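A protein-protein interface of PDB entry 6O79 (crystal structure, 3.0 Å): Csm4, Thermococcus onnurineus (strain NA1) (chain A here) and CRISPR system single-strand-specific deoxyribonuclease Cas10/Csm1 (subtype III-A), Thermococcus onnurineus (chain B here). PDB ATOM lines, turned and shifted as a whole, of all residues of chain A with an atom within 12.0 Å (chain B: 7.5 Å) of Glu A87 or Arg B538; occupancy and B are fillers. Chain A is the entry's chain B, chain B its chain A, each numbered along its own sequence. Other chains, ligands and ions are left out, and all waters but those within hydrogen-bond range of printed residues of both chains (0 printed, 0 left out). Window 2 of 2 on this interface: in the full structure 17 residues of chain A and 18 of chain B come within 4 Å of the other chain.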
ATOM      1  N   LEU A  77      13.754  12.576  -0.600  1.00  0.00           N
ATOM      2  CA  LEU A  77      12.669  11.906  -1.378  1.00  0.00           C
ATOM      3  C   LEU A  77      11.378  12.736  -1.343  1.00  0.00           C
ATOM      4  O   LEU A  77      10.659  12.739  -2.366  1.00  0.00           O
ATOM      5  CB  LEU A  77      12.427  10.501  -0.813  1.00  0.00           C
ATOM      6  CG  LEU A  77      13.518   9.469  -1.104  1.00  0.00           C
ATOM      7  CD1 LEU A  77      13.369   8.252  -0.202  1.00  0.00           C
ATOM      8  CD2 LEU A  77      13.507   9.052  -2.567  1.00  0.00           C
ATOM      9  N   GLU A  78      11.094  13.399  -0.215  1.00  0.00           N
ATOM     10  CA  GLU A  78       9.875  14.227   0.012  1.00  0.00           C
ATOM     11  C   GLU A  78       9.914  15.489  -0.862  1.00  0.00           C
ATOM     12  O   GLU A  78       8.840  15.887  -1.361  1.00  0.00           O
ATOM     13  CB  GLU A  78       9.759  14.588   1.494  1.00  0.00           C
ATOM     14  CG  GLU A  78       9.406  13.401   2.374  1.00  0.00           C
ATOM     15  CD  GLU A  78       9.647  13.603   3.861  1.00  0.00           C
ATOM     16  OE1 GLU A  78       9.898  14.754   4.273  1.00  0.00           O
ATOM     17  OE2 GLU A  78       9.585  12.605   4.605  1.00  0.00           O
ATOM     18  N   ASP A  85       0.165  12.703  -3.538  1.00  0.00           N
ATOM     19  CA  ASP A  85      -0.769  11.713  -2.934  1.00  0.00           C
ATOM     20  C   ASP A  85      -0.030  10.924  -1.845  1.00  0.00           C
ATOM     21  O   ASP A  85       1.006  10.308  -2.169  1.00  0.00           O
ATOM     22  CB  ASP A  85      -1.366  10.794  -4.004  1.00  0.00           C
ATOM     23  CG  ASP A  85      -2.217   9.659  -3.454  1.00  0.00           C
ATOM     24  OD1 ASP A  85      -2.831   9.850  -2.384  1.00  0.00           O
ATOM     25  OD2 ASP A  85      -2.263   8.594  -4.105  1.00  0.00           O
ATOM     26  N   GLU A  86      -0.560  10.936  -0.614  1.00  0.00           N
ATOM     27  CA  GLU A  86       0.031  10.267   0.580  1.00  0.00           C
ATOM     28  C   GLU A  86       0.384   8.817   0.227  1.00  0.00           C
ATOM     29  O   GLU A  86       1.579   8.465   0.297  1.00  0.00           O
ATOM     30  CB  GLU A  86      -0.936  10.274   1.768  1.00  0.00           C
ATOM     31  CG  GLU A  86      -1.297  11.659   2.281  1.00  0.00           C
ATOM     32  CD  GLU A  86      -2.190  11.664   3.512  1.00  0.00           C
ATOM     33  OE1 GLU A  86      -2.161  10.674   4.273  1.00  0.00           O
ATOM     34  OE2 GLU A  86      -2.917  12.659   3.708  1.00  0.00           O
ATOM     35  N   GLU A  87      -0.627   8.027  -0.156  1.00  0.00           N
ATOM     36  CA  GLU A  87      -0.505   6.570  -0.440  1.00  0.00           C
ATOM     37  C   GLU A  87       0.567   6.356  -1.514  1.00  0.00           C
ATOM     38  O   GLU A  87       1.452   5.511  -1.289  1.00  0.00           O
ATOM     39  CB  GLU A  87      -1.857   5.983  -0.853  1.00  0.00           C
ATOM     40  CG  GLU A  87      -2.862   5.934   0.284  1.00  0.00           C
ATOM     41  CD  GLU A  87      -3.973   4.911   0.116  1.00  0.00           C
ATOM     42  OE1 GLU A  87      -4.444   4.732  -1.026  1.00  0.00           O
ATOM     43  OE2 GLU A  87      -4.360   4.290   1.126  1.00  0.00           O
ATOM     44  N   GLU A  88       0.502   7.108  -2.619  1.00  0.00           N
ATOM     45  CA  GLU A  88       1.539   7.105  -3.689  1.00  0.00           C
ATOM     46  C   GLU A  88       2.899   7.459  -3.072  1.00  0.00           C
ATOM     47  O   GLU A  88       3.869   6.723  -3.339  1.00  0.00           O
ATOM     48  CB  GLU A  88       1.175   8.073  -4.818  1.00  0.00           C
ATOM     49  CG  GLU A  88       0.153   7.523  -5.799  1.00  0.00           C
ATOM     50  CD  GLU A  88       0.738   6.850  -7.029  1.00  0.00           C
ATOM     51  OE1 GLU A  88       1.607   5.971  -6.867  1.00  0.00           O
ATOM     52  OE2 GLU A  88       0.329   7.213  -8.150  1.00  0.00           O
ATOM     53  N   ARG A  89       2.956   8.526  -2.260  1.00  0.00           N
ATOM     54  CA  ARG A  89       4.208   9.064  -1.650  1.00  0.00           C
ATOM     55  C   ARG A  89       4.895   7.973  -0.817  1.00  0.00           C
ATOM     56  O   ARG A  89       6.075   7.686  -1.100  1.00  0.00           O
ATOM     57  CB  ARG A  89       3.946  10.317  -0.804  1.00  0.00           C
ATOM     58  CG  ARG A  89       4.468  11.606  -1.428  1.00  0.00           C
ATOM     59  CD  ARG A  89       3.974  12.869  -0.739  1.00  0.00           C
ATOM     60  NE  ARG A  89       4.943  13.457   0.184  1.00  0.00           N
ATOM     61  CZ  ARG A  89       5.706  14.526  -0.061  1.00  0.00           C
ATOM     62  NH1 ARG A  89       5.642  15.164  -1.220  1.00  0.00           N
ATOM     63  NH2 ARG A  89       6.539  14.961   0.869  1.00  0.00           N
ATOM     64  N   TYR A  90       4.195   7.394   0.167  1.00  0.00           N
ATOM     65  CA  TYR A  90       4.716   6.313   1.048  1.00  0.00           C
ATOM     66  C   TYR A  90       5.230   5.159   0.180  1.00  0.00           C
ATOM     67  O   TYR A  90       6.414   4.787   0.313  1.00  0.00           O
ATOM     68  CB  TYR A  90       3.648   5.813   2.027  1.00  0.00           C
ATOM     69  CG  TYR A  90       3.399   6.709   3.215  1.00  0.00           C
ATOM     70  CD1 TYR A  90       4.288   6.753   4.279  1.00  0.00           C
ATOM     71  CD2 TYR A  90       2.266   7.503   3.287  1.00  0.00           C
ATOM     72  CE1 TYR A  90       4.064   7.571   5.375  1.00  0.00           C
ATOM     73  CE2 TYR A  90       2.026   8.326   4.376  1.00  0.00           C
ATOM     74  CZ  TYR A  90       2.928   8.360   5.424  1.00  0.00           C
ATOM     75  OH  TYR A  90       2.697   9.169   6.500  1.00  0.00           O
ATOM     76  N   THR A  91       4.363   4.629  -0.691  1.00  0.00           N
ATOM     77  CA  THR A  91       4.634   3.451  -1.558  1.00  0.00           C
ATOM     78  C   THR A  91       5.850   3.733  -2.449  1.00  0.00           C
ATOM     79  O   THR A  91       6.800   2.929  -2.399  1.00  0.00           O
ATOM     80  CB  THR A  91       3.399   3.057  -2.378  1.00  0.00           C
ATOM     81  OG1 THR A  91       2.910   4.229  -3.031  1.00  0.00           O
ATOM     82  CG2 THR A  91       2.309   2.438  -1.532  1.00  0.00           C
ATOM     83  N   THR A  92       5.834   4.829  -3.217  1.00  0.00           N
ATOM     84  CA  THR A  92       6.948   5.216  -4.127  1.00  0.00           C
ATOM     85  C   THR A  92       8.245   5.306  -3.315  1.00  0.00           C
ATOM     86  O   THR A  92       9.215   4.629  -3.699  1.00  0.00           O
ATOM     87  CB  THR A  92       6.671   6.525  -4.878  1.00  0.00           C
ATOM     88  OG1 THR A  92       6.219   7.497  -3.935  1.00  0.00           O
ATOM     89  CG2 THR A  92       5.656   6.364  -5.990  1.00  0.00           C
ATOM     90  N   ALA A  93       8.245   6.080  -2.224  1.00  0.00           N
ATOM     91  CA  ALA A  93       9.424   6.343  -1.363  1.00  0.00           C
ATOM     92  C   ALA A  93      10.084   5.017  -0.956  1.00  0.00           C
ATOM     93  O   ALA A  93      11.312   4.893  -1.139  1.00  0.00           O
ATOM     94  CB  ALA A  93       9.026   7.154  -0.154  1.00  0.00           C
ATOM     95  N   LYS A  94       9.301   4.066  -0.437  1.00  0.00           N
ATOM     96  CA  LYS A  94       9.800   2.728  -0.012  1.00  0.00           C
ATOM     97  C   LYS A  94      10.495   2.052  -1.202  1.00  0.00           C
ATOM     98  O   LYS A  94      11.651   1.624  -1.032  1.00  0.00           O
ATOM     99  CB  LYS A  94       8.673   1.856   0.553  1.00  0.00           C
ATOM    100  CG  LYS A  94       8.268   2.163   1.990  1.00  0.00           C
ATOM    101  CD  LYS A  94       7.751   0.952   2.745  1.00  0.00           C
ATOM    102  CE  LYS A  94       7.326   1.260   4.165  1.00  0.00           C
ATOM    103  NZ  LYS A  94       5.965   1.847   4.219  1.00  0.00           N
ATOM    104  N   ARG A  95       9.838   1.996  -2.366  1.00  0.00           N
ATOM    105  CA  ARG A  95      10.358   1.300  -3.576  1.00  0.00           C
ATOM    106  C   ARG A  95      11.667   1.962  -4.024  1.00  0.00           C
ATOM    107  O   ARG A  95      12.616   1.215  -4.332  1.00  0.00           O
ATOM    108  CB  ARG A  95       9.320   1.281  -4.704  1.00  0.00           C
ATOM    109  CG  ARG A  95       8.028   0.538  -4.378  1.00  0.00           C
ATOM    110  CD  ARG A  95       8.131  -0.547  -3.315  1.00  0.00           C
ATOM    111  NE  ARG A  95       8.939  -1.694  -3.723  1.00  0.00           N
ATOM    112  CZ  ARG A  95       9.286  -2.706  -2.929  1.00  0.00           C
ATOM    113  NH1 ARG A  95       8.897  -2.735  -1.664  1.00  0.00           N
ATOM    114  NH2 ARG A  95      10.019  -3.696  -3.409  1.00  0.00           N
ATOM    115  N   LEU A  96      11.730   3.299  -4.021  1.00  0.00           N
ATOM    116  CA  LEU A  96      12.955   4.064  -4.384  1.00  0.00           C
ATOM    117  C   LEU A  96      14.040   3.754  -3.345  1.00  0.00           C
ATOM    118  O   LEU A  96      15.196   3.535  -3.749  1.00  0.00           O
ATOM    119  CB  LEU A  96      12.667   5.570  -4.435  1.00  0.00           C
ATOM    120  CG  LEU A  96      11.573   6.058  -5.391  1.00  0.00           C
ATOM    121  CD1 LEU A  96      12.052   7.281  -6.161  1.00  0.00           C
ATOM    122  CD2 LEU A  96      11.114   4.983  -6.366  1.00  0.00           C
ATOM    123  N   ASP B 535       3.008  -8.454   8.461  1.00  0.00           N
ATOM    124  CA  ASP B 535       3.125  -7.008   8.788  1.00  0.00           C
ATOM    125  C   ASP B 535       1.729  -6.388   8.677  1.00  0.00           C
ATOM    126  O   ASP B 535       0.858  -7.019   8.050  1.00  0.00           O
ATOM    127  CB  ASP B 535       4.121  -6.330   7.843  1.00  0.00           C
ATOM    128  CG  ASP B 535       4.543  -4.935   8.269  1.00  0.00           C
ATOM    129  OD1 ASP B 535       5.130  -4.808   9.364  1.00  0.00           O
ATOM    130  OD2 ASP B 535       4.282  -3.985   7.502  1.00  0.00           O
ATOM    131  N   VAL B 536       1.517  -5.208   9.262  1.00  0.00           N
ATOM    132  CA  VAL B 536       0.271  -4.406   9.066  1.00  0.00           C
ATOM    133  C   VAL B 536       0.543  -3.367   7.978  1.00  0.00           C
ATOM    134  O   VAL B 536       1.648  -2.786   7.973  1.00  0.00           O
ATOM    135  CB  VAL B 536      -0.221  -3.758  10.374  1.00  0.00           C
ATOM    136  CG1 VAL B 536      -1.354  -2.771  10.130  1.00  0.00           C
ATOM    137  CG2 VAL B 536      -0.641  -4.815  11.382  1.00  0.00           C
ATOM    138  N   ASP B 537      -0.446  -3.144   7.109  1.00  0.00           N
ATOM    139  CA  ASP B 537      -0.333  -2.309   5.884  1.00  0.00           C
ATOM    140  C   ASP B 537      -0.490  -0.833   6.265  1.00  0.00           C
ATOM    141  O   ASP B 537      -1.420  -0.522   7.036  1.00  0.00           O
ATOM    142  CB  ASP B 537      -1.369  -2.731   4.838  1.00  0.00           C
ATOM    143  CG  ASP B 537      -1.334  -4.214   4.506  1.00  0.00           C
ATOM    144  OD1 ASP B 537      -0.220  -4.767   4.408  1.00  0.00           O
ATOM    145  OD2 ASP B 537      -2.421  -4.805   4.353  1.00  0.00           O
ATOM    146  N   ARG B 538       0.405   0.020   5.751  1.00  0.00           N
ATOM    147  CA  ARG B 538       0.362   1.508   5.833  1.00  0.00           C
ATOM    148  C   ARG B 538       0.055   1.951   7.270  1.00  0.00           C
ATOM    149  O   ARG B 538      -0.877   2.761   7.466  1.00  0.00           O
ATOM    150  CB  ARG B 538      -0.634   2.048   4.801  1.00  0.00           C
ATOM    151  CG  ARG B 538      -0.134   1.927   3.369  1.00  0.00           C
ATOM    152  CD  ARG B 538      -1.233   1.974   2.325  1.00  0.00           C
ATOM    153  NE  ARG B 538      -0.765   1.474   1.036  1.00  0.00           N
ATOM    154  CZ  ARG B 538      -1.542   1.226  -0.016  1.00  0.00           C
ATOM    155  NH1 ARG B 538      -1.004   0.770  -1.136  1.00  0.00           N
ATOM    156  NH2 ARG B 538      -2.848   1.428   0.047  1.00  0.00           N
ATOM    157  N   LEU B 539       0.837   1.444   8.229  1.00  0.00           N
ATOM    158  CA  LEU B 539       0.792   1.834   9.665  1.00  0.00           C
ATOM    159  C   LEU B 539       1.261   3.286   9.804  1.00  0.00           C
ATOM    160  O   LEU B 539       0.598   4.055  10.526  1.00  0.00           O
ATOM    161  CB  LEU B 539       1.688   0.883  10.463  1.00  0.00           C
ATOM    162  CG  LEU B 539       1.717   1.104  11.974  1.00  0.00           C
ATOM    163  CD1 LEU B 539       0.405   0.673  12.613  1.00  0.00           C
ATOM    164  CD2 LEU B 539       2.885   0.358  12.595  1.00  0.00           C
ATOM    165  N   GLY B 540       2.367   3.633   9.137  1.00  0.00           N
ATOM    166  CA  GLY B 540       2.951   4.988   9.122  1.00  0.00           C
ATOM    167  C   GLY B 540       1.891   6.062   8.943  1.00  0.00           C
ATOM    168  O   GLY B 540       1.964   7.082   9.656  1.00  0.00           O
ATOM    169  N   GLU B 541       0.938   5.835   8.031  1.00  0.00           N
ATOM    170  CA  GLU B 541      -0.183   6.765   7.726  1.00  0.00           C
ATOM    171  C   GLU B 541      -1.143   6.808   8.920  1.00  0.00           C
ATOM    172  O   GLU B 541      -1.430   7.921   9.406  1.00  0.00           O
ATOM    173  CB  GLU B 541      -0.905   6.333   6.447  1.00  0.00           C
ATOM    174  CG  GLU B 541      -2.071   7.234   6.071  1.00  0.00           C
ATOM    175  CD  GLU B 541      -2.634   7.022   4.674  1.00  0.00           C
ATOM    176  OE1 GLU B 541      -2.193   6.075   3.990  1.00  0.00           O
ATOM    177  OE2 GLU B 541      -3.514   7.811   4.273  1.00  0.00           O
ATOM    178  N   PHE B 542      -1.616   5.640   9.365  1.00  0.00           N
ATOM    179  CA  PHE B 542      -2.575   5.469  10.490  1.00  0.00           C
ATOM    180  C   PHE B 542      -2.109   6.292  11.699  1.00  0.00           C
ATOM    181  O   PHE B 542      -2.924   7.061  12.247  1.00  0.00           O
ATOM    182  CB  PHE B 542      -2.733   3.986  10.840  1.00  0.00           C
ATOM    183  CG  PHE B 542      -3.508   3.710  12.104  1.00  0.00           C
ATOM    184  CD1 PHE B 542      -4.885   3.866  12.142  1.00  0.00           C
ATOM    185  CD2 PHE B 542      -2.860   3.287  13.256  1.00  0.00           C
ATOM    186  CE1 PHE B 542      -5.595   3.610  13.305  1.00  0.00           C
ATOM    187  CE2 PHE B 542      -3.573   3.030  14.416  1.00  0.00           C
ATOM    188  CZ  PHE B 542      -4.939   3.193  14.440  1.00  0.00           C
ATOM    189  N   PHE B 543      -0.839   6.140  12.089  1.00  0.00           N
ATOM    190  CA  PHE B 543      -0.222   6.838  13.249  1.00  0.00           C
ATOM    191  C   PHE B 543      -0.051   8.330  12.938  1.00  0.00           C
ATOM    192  O   PHE B 543      -0.196   9.152  13.867  1.00  0.00           O
ATOM    193  CB  PHE B 543       1.116   6.199  13.638  1.00  0.00           C
ATOM    194  CG  PHE B 543       1.022   4.889  14.383  1.00  0.00           C
ATOM    195  CD1 PHE B 543      -0.026   4.625  15.255  1.00  0.00           C
ATOM    196  CD2 PHE B 543       2.010   3.928  14.241  1.00  0.00           C
ATOM    197  CE1 PHE B 543      -0.097   3.422  15.941  1.00  0.00           C
ATOM    198  CE2 PHE B 543       1.940   2.727  14.931  1.00  0.00           C
ATOM    199  CZ  PHE B 543       0.886   2.477  15.779  1.00  0.00           C
ATOM    200  N   SER B 544       0.248   8.669  11.680  1.00  0.00           N
ATOM    201  CA  SER B 544       0.441  10.063  11.198  1.00  0.00           C
ATOM    202  C   SER B 544      -0.856  10.869  11.355  1.00  0.00           C
ATOM    203  O   SER B 544      -0.762  12.098  11.540  1.00  0.00           O
ATOM    204  CB  SER B 544       0.936  10.085   9.773  1.00  0.00           C
ATOM    205  OG  SER B 544       0.997  11.415   9.277  1.00  0.00           O
ATOM    206  N   ASP B 602       3.596  -3.993  14.895  1.00  0.00           N
ATOM    207  CA  ASP B 602       2.649  -4.256  13.784  1.00  0.00           C
ATOM    208  C   ASP B 602       3.039  -5.532  13.044  1.00  0.00           C
ATOM    209  O   ASP B 602       2.526  -5.724  11.952  1.00  0.00           O
ATOM    210  CB  ASP B 602       2.611  -3.075  12.816  1.00  0.00           C
ATOM    211  CG  ASP B 602       3.599  -3.173  11.675  1.00  0.00           C
ATOM    212  OD1 ASP B 602       4.772  -2.864  11.888  1.00  0.00           O
ATOM    213  OD2 ASP B 602       3.179  -3.548  10.579  1.00  0.00           O
ATOM    214  N   LEU B 632      -8.399  -1.698   9.227  1.00  0.00           N
ATOM    215  CA  LEU B 632      -6.962  -1.976   8.965  1.00  0.00           C
ATOM    216  C   LEU B 632      -6.821  -3.385   8.383  1.00  0.00           C
ATOM    217  O   LEU B 632      -7.746  -4.201   8.569  1.00  0.00           O
ATOM    218  CB  LEU B 632      -6.164  -1.823  10.263  1.00  0.00           C
ATOM    219  CG  LEU B 632      -6.045  -0.398  10.802  1.00  0.00           C
ATOM    220  CD1 LEU B 632      -5.275  -0.384  12.114  1.00  0.00           C
ATOM    221  CD2 LEU B 632      -5.377   0.523   9.791  1.00  0.00           C
ATOM    222  N   THR B 633      -5.705  -3.644   7.698  1.00  0.00           N
ATOM    223  CA  THR B 633      -5.461  -4.883   6.915  1.00  0.00           C
ATOM    224  C   THR B 633      -4.040  -5.401   7.164  1.00  0.00           C
ATOM    225  O   THR B 633      -3.115  -4.568   7.284  1.00  0.00           O
ATOM    226  CB  THR B 633      -5.701  -4.632   5.422  1.00  0.00           C
ATOM    227  OG1 THR B 633      -4.839  -3.573   5.009  1.00  0.00           O
ATOM    228  CG2 THR B 633      -7.138  -4.274   5.109  1.00  0.00           C
ATOM    229  N   LYS B 662       2.424  -7.128  -0.408  1.00  0.00           N
ATOM    230  CA  LYS B 662       2.256  -5.662  -0.222  1.00  0.00           C
ATOM    231  C   LYS B 662       2.383  -4.983  -1.593  1.00  0.00           C
ATOM    232  O   LYS B 662       1.440  -4.279  -1.996  1.00  0.00           O
ATOM    233  CB  LYS B 662       3.270  -5.128   0.796  1.00  0.00           C
ATOM    234  CG  LYS B 662       3.294  -5.860   2.136  1.00  0.00           C
ATOM    235  CD  LYS B 662       3.949  -5.081   3.261  1.00  0.00           C
ATOM    236  CE  LYS B 662       2.958  -4.357   4.149  1.00  0.00           C
ATOM    237  NZ  LYS B 662       3.513  -3.088   4.673  1.00  0.00           N
ATOM    238  N   ASP B 663       3.487  -5.237  -2.302  1.00  0.00           N
ATOM    239  CA  ASP B 663       3.780  -4.664  -3.647  1.00  0.00           C
ATOM    240  C   ASP B 663       2.602  -4.876  -4.605  1.00  0.00           C
ATOM    241  O   ASP B 663       2.348  -3.962  -5.408  1.00  0.00           O
ATOM    242  CB  ASP B 663       5.047  -5.258  -4.268  1.00  0.00           C
ATOM    243  CG  ASP B 663       6.187  -4.261  -4.339  1.00  0.00           C
ATOM    244  OD1 ASP B 663       6.481  -3.795  -5.457  1.00  0.00           O
ATOM    245  OD2 ASP B 663       6.756  -3.950  -3.277  1.00  0.00           O
ATOM    246  N   GLY B 665      -0.486  -4.613  -4.440  1.00  0.00           N
ATOM    247  CA  GLY B 665      -1.555  -4.086  -3.572  1.00  0.00           C
ATOM    248  C   GLY B 665      -1.459  -4.724  -2.199  1.00  0.00           C
ATOM    249  O   GLY B 665      -0.704  -5.700  -2.066  1.00  0.00           O
ATOM    250  N   ARG B 666      -2.165  -4.197  -1.202  1.00  0.00           N
ATOM    251  CA  ARG B 666      -2.056  -4.670   0.203  1.00  0.00           C
ATOM    252  C   ARG B 666      -3.367  -5.366   0.585  1.00  0.00           C
ATOM    253  O   ARG B 666      -4.270  -5.418  -0.271  1.00  0.00           O
ATOM    254  CB  ARG B 666      -1.649  -3.487   1.085  1.00  0.00           C
ATOM    255  CG  ARG B 666      -0.173  -3.128   0.955  1.00  0.00           C
ATOM    256  CD  ARG B 666       0.134  -1.656   1.168  1.00  0.00           C
ATOM    257  NE  ARG B 666       1.489  -1.444   1.673  1.00  0.00           N
ATOM    258  CZ  ARG B 666       2.561  -1.124   0.941  1.00  0.00           C
ATOM    259  NH1 ARG B 666       3.733  -0.967   1.534  1.00  0.00           N
ATOM    260  NH2 ARG B 666       2.472  -0.958  -0.369  1.00  0.00           N
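O of Glu A87 sits at hydrogen-bond distance from OG1 of Thr A91.
The backbone carbonyl oxygen of Glu A88 is in hydrogen-bond range of the side-chain hydroxyl of Thr A91.
Glu B541 touches Glu A87 (OE1 to CG, 3.8 Å).
O of Gly B540 touches OH of Tyr A90, 3.9 Å away.
Tyr A90 touches Glu B541 (OH to CA, 3.9 Å).
Tyr A90 touches Ser B544 (OH to CB, 3.8 Å).
Thr A91 touches Arg B538.
NH2 of Arg B666 touches CG2 of Thr A91, 3.6 Å away.
OD2 of Asp B663 lies within salt-bridge range of NH1 of Arg A95 (2.9 Å).
The side-chain carboxylate (OE1) of Glu A86 lies close to the side-chain carboxylate (OE2) of Glu B541 (3.2 Å).
OE2 of Glu A87 is in salt-bridge range of NH2 of Arg B538, 3.4 Å away.
No residue of chain A comes within 4 Å of Val B536.
Leu B539 touches none of the printed residues of chain A.
Of chain A, only Tyr A90 (3.9 Å) comes within 4 Å of Gly B540.
No residue of chain A comes within 4 Å of Gly B665.
Of chain A, only Thr A91 (3.6 Å) comes within 4 Å of Arg B666.
Printed residues of chain B within 4 Å of Glu A86: Glu B541.
Of the printed residues of chain A, Asp B663 touches Arg A95 (2.8 Å).
Of the printed residues of chain A, Ser B544 touches Tyr A90.
Printed residues of chain A that touch a printed residue of chain B: Glu A86, Glu A87, Tyr A90, Thr A91 and Arg A95.
Hydrophobic or aromatic side chains of chain A within 4 Å of the printed part of chain B: Tyr A90.
Of the 17 printed residues of chain B, 6 touch a printed residue of chain A.
Printed residues of chain B that touch a printed residue of chain A: Arg B538, Gly B540, Glu B541, Ser B544, Asp B663 and Arg B666.
Among the printed residues, 9 pairs touch across the chains.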
